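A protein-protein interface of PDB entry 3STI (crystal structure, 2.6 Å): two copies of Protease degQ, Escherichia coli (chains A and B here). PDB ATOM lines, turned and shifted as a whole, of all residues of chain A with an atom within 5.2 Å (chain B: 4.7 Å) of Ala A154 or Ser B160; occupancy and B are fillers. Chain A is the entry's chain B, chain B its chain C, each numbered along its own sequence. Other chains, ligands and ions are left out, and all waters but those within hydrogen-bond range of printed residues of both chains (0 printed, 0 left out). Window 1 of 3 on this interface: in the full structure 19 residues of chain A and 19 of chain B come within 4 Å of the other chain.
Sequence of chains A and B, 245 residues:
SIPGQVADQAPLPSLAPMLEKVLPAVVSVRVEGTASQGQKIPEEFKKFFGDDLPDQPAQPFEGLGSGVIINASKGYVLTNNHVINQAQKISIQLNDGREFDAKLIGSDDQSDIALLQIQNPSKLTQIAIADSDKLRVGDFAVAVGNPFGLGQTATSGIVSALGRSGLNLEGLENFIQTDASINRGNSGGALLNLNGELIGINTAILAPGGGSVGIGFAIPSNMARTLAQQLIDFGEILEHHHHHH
The backbone NH (N) of Ser A156 sits at hydrogen-bond distance from the side-chain carboxylate (OD1) of Asp B179 (3.0 Å).
The backbone NH (N) of Ala A154 is in hydrogen-bond range of the backbone carbonyl oxygen (O) of Ser B160 (3.0 Å).
The backbone NH (N) of Ser B160 lies within hydrogen-bond range of the backbone carbonyl oxygen (O) of Gln B177, 2.8 Å away.
The backbone NH (N) of Gly A145 sits at hydrogen-bond distance from the backbone carbonyl oxygen (O) of Thr A153 (2.7 Å).
The backbone NH (N) of Ile B158 is in hydrogen-bond range of the side-chain carboxylate (OD2) of Asp B179, 2.6 Å away.
The backbone carbonyl oxygen of Ile B158 is in hydrogen-bond range of the side-chain hydroxyl of Thr B178 (3.0 Å).
N of Ala A143 lies within hydrogen-bond range of O of Thr A155, 2.8 Å away.
O of Leu A19 lies within hydrogen-bond range of NE2 of Gln A152 (3.0 Å).
Leu A19 touches Val B137.
Gln A152 touches Val B137.
Ser B160 touches Gln A152 (O to O, 3.6 Å).
Thr A153 touches Ser B160 (CA to O, 3.3 Å).
Ala A154 touches Val B137.
Ala A154 touches Ile B158.
Thr A155 touches Asp B179 (CA to OD1, 3.9 Å).
Of chain A, only Gln A152 (3.6 Å), Thr A153 (3.3 Å) and Ala A154 (3.0 Å) come within 4 Å of Ser B160.
Printed residues of chain A within 4 Å of Ile B158: Ala A154.
Of the printed residues of chain B, Ser A156 touches Asp B179.
Thr B178 touches none of the printed residues of chain A.
Ile B215 touches none of the printed residues of chain A.
The nearest residue of chain B that does not touch Ala A154 is Val B159 (4.6 Å).
The nearest printed residue of chain A that does not touch Val B137 is Thr A153 (4.6 Å).
Of the 9 printed residues of chain B, 4 touch a printed residue of chain A.
Hydrophobic or aromatic side chains of chain B within 4 Å of the printed part of chain A: Val B137 and Ile B158.
Among the printed residues, 9 pairs touch across the chains.
Among the printed residues, no Asp or Glu carboxylate lies within 4 Å of a Lys or Arg side-chain nitrogen of the other chain.
No position is printed for both chains.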
ATOM      1  N   LEU A  19     -12.290  27.214 -14.005  1.00  0.00           N
ATOM      2  CA  LEU A  19     -12.450  26.273 -15.119  1.00  0.00           C
ATOM      3  C   LEU A  19     -13.535  26.680 -16.098  1.00  0.00           C
ATOM      4  O   LEU A  19     -13.509  26.247 -17.245  1.00  0.00           O
ATOM      5  CB  LEU A  19     -12.780  24.869 -14.588  1.00  0.00           C
ATOM      6  CG  LEU A  19     -11.638  23.958 -14.187  1.00  0.00           C
ATOM      7  CD1 LEU A  19     -12.168  22.695 -13.591  1.00  0.00           C
ATOM      8  CD2 LEU A  19     -10.740  23.640 -15.342  1.00  0.00           C
ATOM      9  N   VAL A 142      -3.399  22.452 -13.204  1.00  0.00           N
ATOM     10  CA  VAL A 142      -4.691  21.848 -13.565  1.00  0.00           C
ATOM     11  C   VAL A 142      -4.611  21.457 -15.057  1.00  0.00           C
ATOM     12  O   VAL A 142      -4.315  22.313 -15.887  1.00  0.00           O
ATOM     13  CB  VAL A 142      -5.888  22.822 -13.228  1.00  0.00           C
ATOM     14  CG1 VAL A 142      -7.242  22.183 -13.504  1.00  0.00           C
ATOM     15  CG2 VAL A 142      -5.836  23.288 -11.778  1.00  0.00           C
ATOM     16  N   ALA A 143      -4.817  20.172 -15.391  1.00  0.00           N
ATOM     17  CA  ALA A 143      -4.761  19.681 -16.785  1.00  0.00           C
ATOM     18  C   ALA A 143      -6.176  19.540 -17.372  1.00  0.00           C
ATOM     19  O   ALA A 143      -6.943  18.667 -16.952  1.00  0.00           O
ATOM     20  CB  ALA A 143      -4.015  18.347 -16.851  1.00  0.00           C
ATOM     21  N   VAL A 144      -6.535  20.416 -18.327  1.00  0.00           N
ATOM     22  CA  VAL A 144      -7.902  20.420 -18.859  1.00  0.00           C
ATOM     23  C   VAL A 144      -7.995  19.894 -20.288  1.00  0.00           C
ATOM     24  O   VAL A 144      -7.103  20.092 -21.111  1.00  0.00           O
ATOM     25  CB  VAL A 144      -8.621  21.793 -18.720  1.00  0.00           C
ATOM     26  CG1 VAL A 144      -8.608  22.273 -17.276  1.00  0.00           C
ATOM     27  CG2 VAL A 144      -8.014  22.850 -19.632  1.00  0.00           C
ATOM     28  N   GLY A 145      -9.105  19.233 -20.547  1.00  0.00           N
ATOM     29  CA  GLY A 145      -9.412  18.655 -21.841  1.00  0.00           C
ATOM     30  C   GLY A 145     -10.880  18.752 -22.167  1.00  0.00           C
ATOM     31  O   GLY A 145     -11.689  19.174 -21.332  1.00  0.00           O
ATOM     32  N   GLN A 152     -15.992  19.135 -20.435  1.00  0.00           N
ATOM     33  CA  GLN A 152     -14.681  19.379 -19.856  1.00  0.00           C
ATOM     34  C   GLN A 152     -14.188  18.210 -18.968  1.00  0.00           C
ATOM     35  O   GLN A 152     -14.958  17.602 -18.226  1.00  0.00           O
ATOM     36  CB  GLN A 152     -14.763  20.677 -19.034  1.00  0.00           C
ATOM     37  CG  GLN A 152     -13.440  21.373 -18.753  1.00  0.00           C
ATOM     38  CD  GLN A 152     -13.638  22.767 -18.194  1.00  0.00           C
ATOM     39  OE1 GLN A 152     -14.291  22.978 -17.169  1.00  0.00           O
ATOM     40  NE2 GLN A 152     -13.066  23.754 -18.865  1.00  0.00           N
ATOM     41  N   THR A 153     -12.888  17.918 -19.063  1.00  0.00           N
ATOM     42  CA  THR A 153     -12.184  16.923 -18.250  1.00  0.00           C
ATOM     43  C   THR A 153     -11.055  17.666 -17.577  1.00  0.00           C
ATOM     44  O   THR A 153     -10.341  18.407 -18.247  1.00  0.00           O
ATOM     45  CB  THR A 153     -11.699  15.711 -19.064  1.00  0.00           C
ATOM     46  OG1 THR A 153     -12.800  15.154 -19.782  1.00  0.00           O
ATOM     47  CG2 THR A 153     -11.088  14.635 -18.191  1.00  0.00           C
ATOM     48  N   ALA A 154     -10.903  17.508 -16.270  1.00  0.00           N
ATOM     49  CA  ALA A 154      -9.838  18.196 -15.563  1.00  0.00           C
ATOM     50  C   ALA A 154      -9.179  17.299 -14.558  1.00  0.00           C
ATOM     51  O   ALA A 154      -9.833  16.459 -13.944  1.00  0.00           O
ATOM     52  CB  ALA A 154     -10.379  19.445 -14.866  1.00  0.00           C
ATOM     53  N   THR A 155      -7.867  17.465 -14.397  1.00  0.00           N
ATOM     54  CA  THR A 155      -7.079  16.759 -13.387  1.00  0.00           C
ATOM     55  C   THR A 155      -6.309  17.826 -12.665  1.00  0.00           C
ATOM     56  O   THR A 155      -6.112  18.910 -13.210  1.00  0.00           O
ATOM     57  CB  THR A 155      -6.218  15.599 -13.932  1.00  0.00           C
ATOM     58  OG1 THR A 155      -5.127  16.090 -14.693  1.00  0.00           O
ATOM     59  CG2 THR A 155      -7.031  14.540 -14.685  1.00  0.00           C
ATOM     60  N   SER A 156      -5.966  17.569 -11.411  1.00  0.00           N
ATOM     61  CA  SER A 156      -5.282  18.539 -10.575  1.00  0.00           C
ATOM     62  C   SER A 156      -4.010  17.964  -9.947  1.00  0.00           C
ATOM     63  O   SER A 156      -3.878  16.759  -9.714  1.00  0.00           O
ATOM     64  CB  SER A 156      -6.222  19.027  -9.484  1.00  0.00           C
ATOM     65  OG  SER A 156      -5.734  20.243  -8.950  1.00  0.00           O
ATOM     66  N   VAL B 137     -17.303  20.006 -12.552  1.00  0.00           N
ATOM     67  CA  VAL B 137     -15.923  19.567 -12.779  1.00  0.00           C
ATOM     68  C   VAL B 137     -15.036  20.623 -12.107  1.00  0.00           C
ATOM     69  O   VAL B 137     -15.251  21.828 -12.304  1.00  0.00           O
ATOM     70  CB  VAL B 137     -15.600  19.341 -14.284  1.00  0.00           C
ATOM     71  CG1 VAL B 137     -14.107  19.131 -14.524  1.00  0.00           C
ATOM     72  CG2 VAL B 137     -16.411  18.184 -14.856  1.00  0.00           C
ATOM     73  N   ILE B 158     -10.272  15.808  -7.298  1.00  0.00           N
ATOM     74  CA  ILE B 158     -11.338  16.646  -7.824  1.00  0.00           C
ATOM     75  C   ILE B 158     -12.301  15.818  -8.662  1.00  0.00           C
ATOM     76  O   ILE B 158     -11.957  14.709  -9.074  1.00  0.00           O
ATOM     77  CB  ILE B 158     -10.779  17.849  -8.665  1.00  0.00           C
ATOM     78  CG1 ILE B 158     -10.057  17.412  -9.978  1.00  0.00           C
ATOM     79  CG2 ILE B 158      -9.963  18.841  -7.829  1.00  0.00           C
ATOM     80  CD1 ILE B 158     -10.186  18.362 -11.104  1.00  0.00           C
ATOM     81  N   VAL B 159     -13.505  16.370  -8.917  1.00  0.00           N
ATOM     82  CA  VAL B 159     -14.487  15.818  -9.853  1.00  0.00           C
ATOM     83  C   VAL B 159     -13.864  16.117 -11.220  1.00  0.00           C
ATOM     84  O   VAL B 159     -13.644  17.288 -11.526  1.00  0.00           O
ATOM     85  CB  VAL B 159     -15.920  16.418  -9.670  1.00  0.00           C
ATOM     86  CG1 VAL B 159     -16.862  15.969 -10.787  1.00  0.00           C
ATOM     87  CG2 VAL B 159     -16.506  16.093  -8.291  1.00  0.00           C
ATOM     88  N   SER B 160     -13.465  15.081 -11.959  1.00  0.00           N
ATOM     89  CA  SER B 160     -12.741  15.199 -13.223  1.00  0.00           C
ATOM     90  C   SER B 160     -13.661  15.341 -14.433  1.00  0.00           C
ATOM     91  O   SER B 160     -13.361  16.148 -15.306  1.00  0.00           O
ATOM     92  CB  SER B 160     -11.796  14.011 -13.417  1.00  0.00           C
ATOM     93  OG  SER B 160     -11.781  13.534 -14.756  1.00  0.00           O
ATOM     94  N   ALA B 161     -14.721  14.509 -14.526  1.00  0.00           N
ATOM     95  CA  ALA B 161     -15.701  14.526 -15.619  1.00  0.00           C
ATOM     96  C   ALA B 161     -17.049  14.029 -15.128  1.00  0.00           C
ATOM     97  O   ALA B 161     -17.109  13.280 -14.150  1.00  0.00           O
ATOM     98  CB  ALA B 161     -15.211  13.671 -16.778  1.00  0.00           C
ATOM     99  N   GLN B 177     -16.540  10.844 -12.726  1.00  0.00           N
ATOM    100  CA  GLN B 177     -15.107  10.620 -12.869  1.00  0.00           C
ATOM    101  C   GLN B 177     -14.367  11.473 -11.852  1.00  0.00           C
ATOM    102  O   GLN B 177     -14.772  12.593 -11.562  1.00  0.00           O
ATOM    103  CB  GLN B 177     -14.627  10.926 -14.295  1.00  0.00           C
ATOM    104  CG  GLN B 177     -14.496   9.684 -15.150  1.00  0.00           C
ATOM    105  CD  GLN B 177     -14.169  10.028 -16.573  1.00  0.00           C
ATOM    106  OE1 GLN B 177     -15.030   9.950 -17.455  1.00  0.00           O
ATOM    107  NE2 GLN B 177     -12.924  10.419 -16.830  1.00  0.00           N
ATOM    108  N   THR B 178     -13.292  10.930 -11.302  1.00  0.00           N
ATOM    109  CA  THR B 178     -12.488  11.600 -10.279  1.00  0.00           C
ATOM    110  C   THR B 178     -11.013  11.220 -10.465  1.00  0.00           C
ATOM    111  O   THR B 178     -10.720  10.131 -10.961  1.00  0.00           O
ATOM    112  CB  THR B 178     -13.041  11.281  -8.854  1.00  0.00           C
ATOM    113  OG1 THR B 178     -12.320  12.022  -7.886  1.00  0.00           O
ATOM    114  CG2 THR B 178     -13.008   9.807  -8.499  1.00  0.00           C
ATOM    115  N   ASP B 179     -10.093  12.131 -10.100  1.00  0.00           N
ATOM    116  CA  ASP B 179      -8.649  11.884 -10.189  1.00  0.00           C
ATOM    117  C   ASP B 179      -8.142  11.400  -8.811  1.00  0.00           C
ATOM    118  O   ASP B 179      -6.955  11.147  -8.639  1.00  0.00           O
ATOM    119  CB  ASP B 179      -7.877  13.114 -10.724  1.00  0.00           C
ATOM    120  CG  ASP B 179      -7.879  14.325  -9.814  1.00  0.00           C
ATOM    121  OD1 ASP B 179      -6.919  15.123  -9.884  1.00  0.00           O
ATOM    122  OD2 ASP B 179      -8.814  14.449  -8.999  1.00  0.00           O
ATOM    123  N   ILE B 215      -7.678   8.096 -13.604  1.00  0.00           N
ATOM    124  CA  ILE B 215      -9.060   8.513 -13.356  1.00  0.00           C
ATOM    125  C   ILE B 215      -9.870   7.361 -12.763  1.00  0.00           C
ATOM    126  O   ILE B 215      -9.748   6.210 -13.196  1.00  0.00           O
ATOM    127  CB  ILE B 215      -9.767   9.077 -14.621  1.00  0.00           C
ATOM    128  CG1 ILE B 215      -8.765   9.618 -15.654  1.00  0.00           C
ATOM    129  CG2 ILE B 215     -10.801  10.145 -14.244  1.00  0.00           C
ATOM    130  CD1 ILE B 215      -9.014   9.136 -17.016  1.00  0.00           C
